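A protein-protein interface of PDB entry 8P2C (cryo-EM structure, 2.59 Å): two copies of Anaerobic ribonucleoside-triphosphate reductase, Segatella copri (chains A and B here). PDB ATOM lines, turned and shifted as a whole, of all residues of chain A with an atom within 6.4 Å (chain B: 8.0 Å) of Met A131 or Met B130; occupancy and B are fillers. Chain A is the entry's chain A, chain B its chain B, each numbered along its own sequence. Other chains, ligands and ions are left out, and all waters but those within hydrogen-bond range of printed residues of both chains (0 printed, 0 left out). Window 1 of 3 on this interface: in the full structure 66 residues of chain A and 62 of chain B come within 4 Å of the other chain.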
ATOM      1  N   PRO A 126     -12.983 -18.744 -24.133  1.00  0.00           N
ATOM      2  CA  PRO A 126     -13.310 -20.040 -23.516  1.00  0.00           C
ATOM      3  C   PRO A 126     -14.755 -20.172 -23.056  1.00  0.00           C
ATOM      4  O   PRO A 126     -15.327 -21.266 -23.146  1.00  0.00           O
ATOM      5  CB  PRO A 126     -12.328 -20.104 -22.342  1.00  0.00           C
ATOM      6  CG  PRO A 126     -11.142 -19.355 -22.832  1.00  0.00           C
ATOM      7  CD  PRO A 126     -11.674 -18.238 -23.682  1.00  0.00           C
ATOM      8  N   ALA A 127     -15.367 -19.088 -22.573  1.00  0.00           N
ATOM      9  CA  ALA A 127     -16.756 -19.159 -22.133  1.00  0.00           C
ATOM     10  C   ALA A 127     -17.696 -19.474 -23.292  1.00  0.00           C
ATOM     11  O   ALA A 127     -18.627 -20.275 -23.147  1.00  0.00           O
ATOM     12  CB  ALA A 127     -17.158 -17.852 -21.456  1.00  0.00           C
ATOM     13  N   GLY A 128     -17.472 -18.849 -24.449  1.00  0.00           N
ATOM     14  CA  GLY A 128     -18.310 -19.135 -25.601  1.00  0.00           C
ATOM     15  C   GLY A 128     -18.183 -20.570 -26.071  1.00  0.00           C
ATOM     16  O   GLY A 128     -19.181 -21.220 -26.398  1.00  0.00           O
ATOM     17  N   MET A 129     -16.953 -21.084 -26.108  1.00  0.00           N
ATOM     18  CA  MET A 129     -16.745 -22.475 -26.483  1.00  0.00           C
ATOM     19  C   MET A 129     -17.391 -23.426 -25.486  1.00  0.00           C
ATOM     20  O   MET A 129     -17.931 -24.463 -25.886  1.00  0.00           O
ATOM     21  CB  MET A 129     -15.252 -22.769 -26.605  1.00  0.00           C
ATOM     22  CG  MET A 129     -14.562 -22.029 -27.731  1.00  0.00           C
ATOM     23  SD  MET A 129     -12.819 -22.469 -27.859  1.00  0.00           S
ATOM     24  CE  MET A 129     -12.352 -21.598 -29.351  1.00  0.00           C
ATOM     25  N   MET A 130     -17.358 -23.094 -24.196  1.00  0.00           N
ATOM     26  CA  MET A 130     -17.982 -23.950 -23.199  1.00  0.00           C
ATOM     27  C   MET A 130     -19.501 -23.842 -23.184  1.00  0.00           C
ATOM     28  O   MET A 130     -20.164 -24.766 -22.708  1.00  0.00           O
ATOM     29  CB  MET A 130     -17.425 -23.632 -21.813  1.00  0.00           C
ATOM     30  CG  MET A 130     -16.001 -24.100 -21.617  1.00  0.00           C
ATOM     31  SD  MET A 130     -15.872 -25.896 -21.600  1.00  0.00           S
ATOM     32  CE  MET A 130     -14.307 -26.125 -22.428  1.00  0.00           C
ATOM     33  N   MET A 131     -20.072 -22.759 -23.698  1.00  0.00           N
ATOM     34  CA  MET A 131     -21.523 -22.677 -23.813  1.00  0.00           C
ATOM     35  C   MET A 131     -22.057 -23.327 -25.080  1.00  0.00           C
ATOM     36  O   MET A 131     -23.168 -23.879 -25.067  1.00  0.00           O
ATOM     37  CB  MET A 131     -21.978 -21.215 -23.764  1.00  0.00           C
ATOM     38  CG  MET A 131     -21.842 -20.555 -22.398  1.00  0.00           C
ATOM     39  SD  MET A 131     -23.141 -21.016 -21.231  1.00  0.00           S
ATOM     40  CE  MET A 131     -22.366 -22.360 -20.341  1.00  0.00           C
ATOM     41  N   LYS A 132     -21.283 -23.286 -26.169  1.00  0.00           N
ATOM     42  CA  LYS A 132     -21.700 -23.958 -27.394  1.00  0.00           C
ATOM     43  C   LYS A 132     -21.843 -25.459 -27.181  1.00  0.00           C
ATOM     44  O   LYS A 132     -22.812 -26.071 -27.655  1.00  0.00           O
ATOM     45  CB  LYS A 132     -20.706 -23.668 -28.516  1.00  0.00           C
ATOM     46  CG  LYS A 132     -20.732 -22.239 -29.011  1.00  0.00           C
ATOM     47  CD  LYS A 132     -19.761 -22.041 -30.160  1.00  0.00           C
ATOM     48  CE  LYS A 132     -20.108 -22.941 -31.334  1.00  0.00           C
ATOM     49  NZ  LYS A 132     -21.470 -22.661 -31.865  1.00  0.00           N
ATOM     50  N   PHE A 133     -20.892 -26.069 -26.472  1.00  0.00           N
ATOM     51  CA  PHE A 133     -20.978 -27.500 -26.204  1.00  0.00           C
ATOM     52  C   PHE A 133     -22.232 -27.837 -25.414  1.00  0.00           C
ATOM     53  O   PHE A 133     -22.919 -28.819 -25.717  1.00  0.00           O
ATOM     54  CB  PHE A 133     -19.736 -27.974 -25.449  1.00  0.00           C
ATOM     55  CG  PHE A 133     -18.467 -27.847 -26.230  1.00  0.00           C
ATOM     56  CD1 PHE A 133     -18.448 -28.090 -27.589  1.00  0.00           C
ATOM     57  CD2 PHE A 133     -17.291 -27.475 -25.606  1.00  0.00           C
ATOM     58  CE1 PHE A 133     -17.281 -27.970 -28.308  1.00  0.00           C
ATOM     59  CE2 PHE A 133     -16.123 -27.350 -26.322  1.00  0.00           C
ATOM     60  CZ  PHE A 133     -16.121 -27.592 -27.675  1.00  0.00           C
ATOM     61  N   ALA A 134     -22.549 -27.033 -24.398  1.00  0.00           N
ATOM     62  CA  ALA A 134     -23.734 -27.297 -23.590  1.00  0.00           C
ATOM     63  C   ALA A 134     -25.006 -27.190 -24.420  1.00  0.00           C
ATOM     64  O   ALA A 134     -25.885 -28.058 -24.336  1.00  0.00           O
ATOM     65  CB  ALA A 134     -23.781 -26.339 -22.402  1.00  0.00           C
ATOM     66  N   SER A 135     -25.120 -26.144 -25.240  1.00  0.00           N
ATOM     67  CA  SER A 135     -26.322 -25.996 -26.059  1.00  0.00           C
ATOM     68  C   SER A 135     -26.472 -27.155 -27.039  1.00  0.00           C
ATOM     69  O   SER A 135     -27.570 -27.719 -27.195  1.00  0.00           O
ATOM     70  CB  SER A 135     -26.288 -24.663 -26.803  1.00  0.00           C
ATOM     71  OG  SER A 135     -25.156 -24.581 -27.650  1.00  0.00           O
ATOM     72  N   GLU A 136     -25.374 -27.530 -27.702  1.00  0.00           N
ATOM     73  CA  GLU A 136     -25.430 -28.599 -28.688  1.00  0.00           C
ATOM     74  C   GLU A 136     -25.714 -29.949 -28.050  1.00  0.00           C
ATOM     75  O   GLU A 136     -26.385 -30.788 -28.659  1.00  0.00           O
ATOM     76  CB  GLU A 136     -24.128 -28.647 -29.483  1.00  0.00           C
ATOM     77  CG  GLU A 136     -23.878 -27.417 -30.332  1.00  0.00           C
ATOM     78  CD  GLU A 136     -24.903 -27.246 -31.436  1.00  0.00           C
ATOM     79  OE1 GLU A 136     -25.469 -28.262 -31.890  1.00  0.00           O
ATOM     80  OE2 GLU A 136     -25.143 -26.093 -31.851  1.00  0.00           O
ATOM     81  N   THR A 138     -27.488 -30.307 -25.326  1.00  0.00           N
ATOM     82  CA  THR A 138     -28.807 -30.263 -24.709  1.00  0.00           C
ATOM     83  C   THR A 138     -29.941 -30.387 -25.722  1.00  0.00           C
ATOM     84  O   THR A 138     -30.943 -31.052 -25.438  1.00  0.00           O
ATOM     85  CB  THR A 138     -28.959 -28.968 -23.907  1.00  0.00           C
ATOM     86  OG1 THR A 138     -28.221 -29.075 -22.684  1.00  0.00           O
ATOM     87  CG2 THR A 138     -30.413 -28.693 -23.588  1.00  0.00           C
ATOM     88  N   ASP A 166     -32.271 -24.721 -25.750  1.00  0.00           N
ATOM     89  CA  ASP A 166     -31.094 -25.213 -25.047  1.00  0.00           C
ATOM     90  C   ASP A 166     -31.193 -25.044 -23.539  1.00  0.00           C
ATOM     91  O   ASP A 166     -30.393 -25.640 -22.813  1.00  0.00           O
ATOM     92  CB  ASP A 166     -29.843 -24.506 -25.569  1.00  0.00           C
ATOM     93  CG  ASP A 166     -30.012 -23.004 -25.646  1.00  0.00           C
ATOM     94  OD1 ASP A 166     -31.116 -22.511 -25.339  1.00  0.00           O
ATOM     95  OD2 ASP A 166     -29.039 -22.314 -26.014  1.00  0.00           O
ATOM     96  N   TYR A 167     -32.139 -24.243 -23.053  1.00  0.00           N
ATOM     97  CA  TYR A 167     -32.366 -24.059 -21.629  1.00  0.00           C
ATOM     98  C   TYR A 167     -33.589 -24.819 -21.133  1.00  0.00           C
ATOM     99  O   TYR A 167     -34.077 -24.540 -20.037  1.00  0.00           O
ATOM    100  CB  TYR A 167     -32.504 -22.572 -21.304  1.00  0.00           C
ATOM    101  CG  TYR A 167     -31.194 -21.880 -20.994  1.00  0.00           C
ATOM    102  CD1 TYR A 167     -30.418 -21.337 -22.005  1.00  0.00           C
ATOM    103  CD2 TYR A 167     -30.738 -21.770 -19.689  1.00  0.00           C
ATOM    104  CE1 TYR A 167     -29.223 -20.706 -21.724  1.00  0.00           C
ATOM    105  CE2 TYR A 167     -29.548 -21.141 -19.399  1.00  0.00           C
ATOM    106  CZ  TYR A 167     -28.794 -20.612 -20.419  1.00  0.00           C
ATOM    107  OH  TYR A 167     -27.605 -19.984 -20.135  1.00  0.00           O
ATOM    108  N   PRO A 169     -34.050 -28.183 -20.178  1.00  0.00           N
ATOM    109  CA  PRO A 169     -33.876 -28.972 -18.945  1.00  0.00           C
ATOM    110  C   PRO A 169     -33.681 -28.131 -17.700  1.00  0.00           C
ATOM    111  O   PRO A 169     -34.013 -28.593 -16.602  1.00  0.00           O
ATOM    112  CB  PRO A 169     -32.639 -29.829 -19.242  1.00  0.00           C
ATOM    113  CG  PRO A 169     -31.965 -29.163 -20.365  1.00  0.00           C
ATOM    114  CD  PRO A 169     -33.045 -28.557 -21.187  1.00  0.00           C
ATOM    115  N   THR A 170     -33.150 -26.919 -17.826  1.00  0.00           N
ATOM    116  CA  THR A 170     -33.089 -25.976 -16.716  1.00  0.00           C
ATOM    117  C   THR A 170     -34.419 -25.236 -16.672  1.00  0.00           C
ATOM    118  O   THR A 170     -34.680 -24.368 -17.510  1.00  0.00           O
ATOM    119  CB  THR A 170     -31.926 -25.004 -16.888  1.00  0.00           C
ATOM    120  OG1 THR A 170     -32.229 -24.081 -17.939  1.00  0.00           O
ATOM    121  CG2 THR A 170     -30.659 -25.754 -17.243  1.00  0.00           C
ATOM    122  N   GLN A 313     -21.274 -12.953 -23.282  1.00  0.00           N
ATOM    123  CA  GLN A 313     -22.485 -12.192 -23.566  1.00  0.00           C
ATOM    124  C   GLN A 313     -22.766 -11.185 -22.459  1.00  0.00           C
ATOM    125  O   GLN A 313     -22.712 -11.515 -21.275  1.00  0.00           O
ATOM    126  CB  GLN A 313     -23.681 -13.130 -23.738  1.00  0.00           C
ATOM    127  CG  GLN A 313     -23.523 -14.137 -24.865  1.00  0.00           C
ATOM    128  CD  GLN A 313     -24.699 -15.086 -24.965  1.00  0.00           C
ATOM    129  OE1 GLN A 313     -25.627 -15.031 -24.158  1.00  0.00           O
ATOM    130  NE2 GLN A 313     -24.667 -15.966 -25.959  1.00  0.00           N
ATOM    131  N   MET B 104     -27.922 -36.152 -16.752  1.00  0.00           N
ATOM    132  CA  MET B 104     -26.493 -36.251 -16.482  1.00  0.00           C
ATOM    133  C   MET B 104     -25.998 -37.688 -16.533  1.00  0.00           C
ATOM    134  O   MET B 104     -24.840 -37.927 -16.892  1.00  0.00           O
ATOM    135  CB  MET B 104     -26.170 -35.633 -15.121  1.00  0.00           C
ATOM    136  CG  MET B 104     -26.400 -34.132 -15.048  1.00  0.00           C
ATOM    137  SD  MET B 104     -25.396 -33.217 -16.234  1.00  0.00           S
ATOM    138  CE  MET B 104     -23.755 -33.772 -15.786  1.00  0.00           C
ATOM    139  N   ASP B 124     -28.018 -27.070  -9.571  1.00  0.00           N
ATOM    140  CA  ASP B 124     -29.394 -26.603  -9.463  1.00  0.00           C
ATOM    141  C   ASP B 124     -29.577 -25.286 -10.211  1.00  0.00           C
ATOM    142  O   ASP B 124     -30.565 -25.097 -10.923  1.00  0.00           O
ATOM    143  CB  ASP B 124     -29.795 -26.444  -7.995  1.00  0.00           C
ATOM    144  CG  ASP B 124     -28.823 -25.582  -7.212  1.00  0.00           C
ATOM    145  OD1 ASP B 124     -27.627 -25.558  -7.568  1.00  0.00           O
ATOM    146  OD2 ASP B 124     -29.257 -24.929  -6.239  1.00  0.00           O
ATOM    147  N   THR B 125     -28.623 -24.380 -10.042  1.00  0.00           N
ATOM    148  CA  THR B 125     -28.628 -23.145 -10.805  1.00  0.00           C
ATOM    149  C   THR B 125     -28.425 -23.462 -12.285  1.00  0.00           C
ATOM    150  O   THR B 125     -27.614 -24.332 -12.625  1.00  0.00           O
ATOM    151  CB  THR B 125     -27.526 -22.211 -10.301  1.00  0.00           C
ATOM    152  OG1 THR B 125     -27.666 -22.027  -8.888  1.00  0.00           O
ATOM    153  CG2 THR B 125     -27.596 -20.856 -10.985  1.00  0.00           C
ATOM    154  N   PRO B 126     -29.156 -22.801 -13.189  1.00  0.00           N
ATOM    155  CA  PRO B 126     -29.012 -23.120 -14.620  1.00  0.00           C
ATOM    156  C   PRO B 126     -27.590 -23.010 -15.149  1.00  0.00           C
ATOM    157  O   PRO B 126     -27.168 -23.853 -15.953  1.00  0.00           O
ATOM    158  CB  PRO B 126     -29.945 -22.104 -15.287  1.00  0.00           C
ATOM    159  CG  PRO B 126     -30.987 -21.843 -14.264  1.00  0.00           C
ATOM    160  CD  PRO B 126     -30.305 -21.916 -12.932  1.00  0.00           C
ATOM    161  N   ALA B 127     -26.834 -21.999 -14.714  1.00  0.00           N
ATOM    162  CA  ALA B 127     -25.468 -21.837 -15.202  1.00  0.00           C
ATOM    163  C   ALA B 127     -24.593 -23.017 -14.799  1.00  0.00           C
ATOM    164  O   ALA B 127     -23.790 -23.510 -15.604  1.00  0.00           O
ATOM    165  CB  ALA B 127     -24.881 -20.526 -14.687  1.00  0.00           C
ATOM    166  N   GLY B 128     -24.737 -23.488 -13.561  1.00  0.00           N
ATOM    167  CA  GLY B 128     -23.973 -24.646 -13.129  1.00  0.00           C
ATOM    168  C   GLY B 128     -24.313 -25.896 -13.916  1.00  0.00           C
ATOM    169  O   GLY B 128     -23.427 -26.680 -14.271  1.00  0.00           O
ATOM    170  N   MET B 129     -25.601 -26.100 -14.202  1.00  0.00           N
ATOM    171  CA  MET B 129     -26.007 -27.255 -14.993  1.00  0.00           C
ATOM    172  C   MET B 129     -25.428 -27.188 -16.400  1.00  0.00           C
ATOM    173  O   MET B 129     -24.954 -28.200 -16.934  1.00  0.00           O
ATOM    174  CB  MET B 129     -27.531 -27.348 -15.037  1.00  0.00           C
ATOM    175  CG  MET B 129     -28.050 -28.668 -15.578  1.00  0.00           C
ATOM    176  SD  MET B 129     -29.845 -28.801 -15.502  1.00  0.00           S
ATOM    177  CE  MET B 129     -30.133 -28.512 -13.761  1.00  0.00           C
ATOM    178  N   MET B 130     -25.448 -26.003 -17.014  1.00  0.00           N
ATOM    179  CA  MET B 130     -24.871 -25.864 -18.349  1.00  0.00           C
ATOM    180  C   MET B 130     -23.369 -26.124 -18.333  1.00  0.00           C
ATOM    181  O   MET B 130     -22.831 -26.775 -19.239  1.00  0.00           O
ATOM    182  CB  MET B 130     -25.177 -24.477 -18.910  1.00  0.00           C
ATOM    183  CG  MET B 130     -26.661 -24.196 -19.074  1.00  0.00           C
ATOM    184  SD  MET B 130     -27.460 -25.207 -20.335  1.00  0.00           S
ATOM    185  CE  MET B 130     -26.876 -24.413 -21.825  1.00  0.00           C
ATOM    186  N   MET B 131     -22.673 -25.633 -17.304  1.00  0.00           N
ATOM    187  CA  MET B 131     -21.237 -25.876 -17.211  1.00  0.00           C
ATOM    188  C   MET B 131     -20.932 -27.357 -17.020  1.00  0.00           C
ATOM    189  O   MET B 131     -19.964 -27.878 -17.587  1.00  0.00           O
ATOM    190  CB  MET B 131     -20.636 -25.047 -16.079  1.00  0.00           C
ATOM    191  CG  MET B 131     -20.565 -23.562 -16.386  1.00  0.00           C
ATOM    192  SD  MET B 131     -19.733 -23.231 -17.952  1.00  0.00           S
ATOM    193  CE  MET B 131     -19.723 -21.441 -17.959  1.00  0.00           C
ATOM    194  N   LYS B 132     -21.742 -28.052 -16.216  1.00  0.00           N
ATOM    195  CA  LYS B 132     -21.561 -29.491 -16.054  1.00  0.00           C
ATOM    196  C   LYS B 132     -21.777 -30.226 -17.371  1.00  0.00           C
ATOM    197  O   LYS B 132     -21.016 -31.141 -17.714  1.00  0.00           O
ATOM    198  CB  LYS B 132     -22.508 -30.024 -14.980  1.00  0.00           C
ATOM    199  CG  LYS B 132     -22.176 -29.570 -13.573  1.00  0.00           C
ATOM    200  CD  LYS B 132     -20.802 -30.058 -13.144  1.00  0.00           C
ATOM    201  CE  LYS B 132     -20.485 -29.635 -11.719  1.00  0.00           C
ATOM    202  NZ  LYS B 132     -20.494 -28.154 -11.564  1.00  0.00           N
ATOM    203  N   PHE B 133     -22.817 -29.841 -18.116  1.00  0.00           N
ATOM    204  CA  PHE B 133     -23.035 -30.415 -19.441  1.00  0.00           C
ATOM    205  C   PHE B 133     -21.805 -30.234 -20.318  1.00  0.00           C
ATOM    206  O   PHE B 133     -21.349 -31.178 -20.976  1.00  0.00           O
ATOM    207  CB  PHE B 133     -24.254 -29.767 -20.099  1.00  0.00           C
ATOM    208  CG  PHE B 133     -25.562 -30.376 -19.694  1.00  0.00           C
ATOM    209  CD1 PHE B 133     -25.718 -31.748 -19.643  1.00  0.00           C
ATOM    210  CD2 PHE B 133     -26.638 -29.572 -19.365  1.00  0.00           C
ATOM    211  CE1 PHE B 133     -26.922 -32.307 -19.273  1.00  0.00           C
ATOM    212  CE2 PHE B 133     -27.842 -30.126 -18.992  1.00  0.00           C
ATOM    213  CZ  PHE B 133     -27.985 -31.494 -18.945  1.00  0.00           C
ATOM    214  N   ALA B 134     -21.248 -29.022 -20.327  1.00  0.00           N
ATOM    215  CA  ALA B 134     -20.084 -28.746 -21.163  1.00  0.00           C
ATOM    216  C   ALA B 134     -18.890 -29.599 -20.758  1.00  0.00           C
ATOM    217  O   ALA B 134     -18.200 -30.165 -21.616  1.00  0.00           O
ATOM    218  CB  ALA B 134     -19.725 -27.268 -21.084  1.00  0.00           C
ATOM    219  N   SER B 135     -18.623 -29.695 -19.454  1.00  0.00           N
ATOM    220  CA  SER B 135     -17.467 -30.458 -18.991  1.00  0.00           C
ATOM    221  C   SER B 135     -17.599 -31.933 -19.345  1.00  0.00           C
ATOM    222  O   SER B 135     -16.637 -32.557 -19.826  1.00  0.00           O
ATOM    223  CB  SER B 135     -17.298 -30.281 -17.483  1.00  0.00           C
ATOM    224  OG  SER B 135     -16.165 -30.989 -17.011  1.00  0.00           O
ATOM    225  N   GLU B 136     -18.783 -32.509 -19.116  1.00  0.00           N
ATOM    226  CA  GLU B 136     -18.987 -33.917 -19.429  1.00  0.00           C
ATOM    227  C   GLU B 136     -18.965 -34.180 -20.925  1.00  0.00           C
ATOM    228  O   GLU B 136     -18.574 -35.274 -21.340  1.00  0.00           O
ATOM    229  CB  GLU B 136     -20.305 -34.407 -18.831  1.00  0.00           C
ATOM    230  CG  GLU B 136     -20.411 -34.226 -17.327  1.00  0.00           C
ATOM    231  CD  GLU B 136     -19.346 -34.986 -16.562  1.00  0.00           C
ATOM    232  OE1 GLU B 136     -18.898 -36.046 -17.049  1.00  0.00           O
ATOM    233  OE2 GLU B 136     -18.957 -34.521 -15.471  1.00  0.00           O
ATOM    234  N   THR B 137     -19.378 -33.213 -21.743  1.00  0.00           N
ATOM    235  CA  THR B 137     -19.263 -33.383 -23.185  1.00  0.00           C
ATOM    236  C   THR B 137     -17.816 -33.298 -23.652  1.00  0.00           C
ATOM    237  O   THR B 137     -17.420 -34.027 -24.568  1.00  0.00           O
ATOM    238  CB  THR B 137     -20.107 -32.330 -23.904  1.00  0.00           C
ATOM    239  OG1 THR B 137     -21.458 -32.399 -23.434  1.00  0.00           O
ATOM    240  CG2 THR B 137     -20.088 -32.560 -25.404  1.00  0.00           C
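Hydrophobic or aromatic side chains of chain A within 4 Å of the printed part of chain B: Met A131 and Ala A134.
Of the 15 printed residues of chain B, 6 touch a printed residue of chain A.
Hydrophobic or aromatic side chains of chain B within 4 Å of the printed part of chain A: Pro B126, Met B129, Met B130, Met B131, Phe B133 and Ala B134.
Among the printed residues, no Asp or Glu carboxylate lies within 4 Å of a Lys or Arg side-chain nitrogen of the other chain.
Met A131 touches two residues of chain B.
Printed residues of chain A within 4 Å of Met B130: Met A131, Ala A134 and Asp A166.
Printed residues of chain A within 4 Å of Met B131: Met A131.
Printed residues of chain A within 4 Å of Ala B134: Met A130 (3.0 Å).
Of the printed residues of chain B, Thr A138 touches Phe B133.
Lys A132 touches none of the printed residues of chain B.
The nearest residue of chain B that does not touch Met A131 is Ala B127 (5.1 Å).
O of Met A131 sits at hydrogen-bond distance from OG of Ser A135 (3.3 Å).
The backbone carbonyl oxygen (O) of Ala A134 lies within hydrogen-bond range of the side-chain hydroxyl (OG1) of Thr A138, 3.0 Å away.
The side-chain hydroxyl (OG1) of Thr A170 sits at hydrogen-bond distance from the backbone carbonyl oxygen (O) of Tyr A167.
The backbone carbonyl oxygen of Phe B133 lies within hydrogen-bond range of the side-chain hydroxyl of Thr B137 (2.7 Å).
Among the printed residues, merely in contact across the chains: Met A130 with Ala B134, Met A131 with Met B130, Met A131 with Met B131, Ala A134 with Met B130, Thr A138 with Phe B133, Asp A166 with Met B130, Thr A170 with Pro B126 and Thr A170 with Met B129.
Met A130 touches Ala B134, and with the chains exchanged Ala A134 touches Met B130.
Met A131 touches Met B130, but with the chains exchanged Met A130 does not touch Met B131 (4.5 Å).
Met A131 touches its own counterpart, Met B131.
Positions printed for both chains: 126, 127, 128, 129, 130, 131, 132, 133, 134, 135 and 136.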
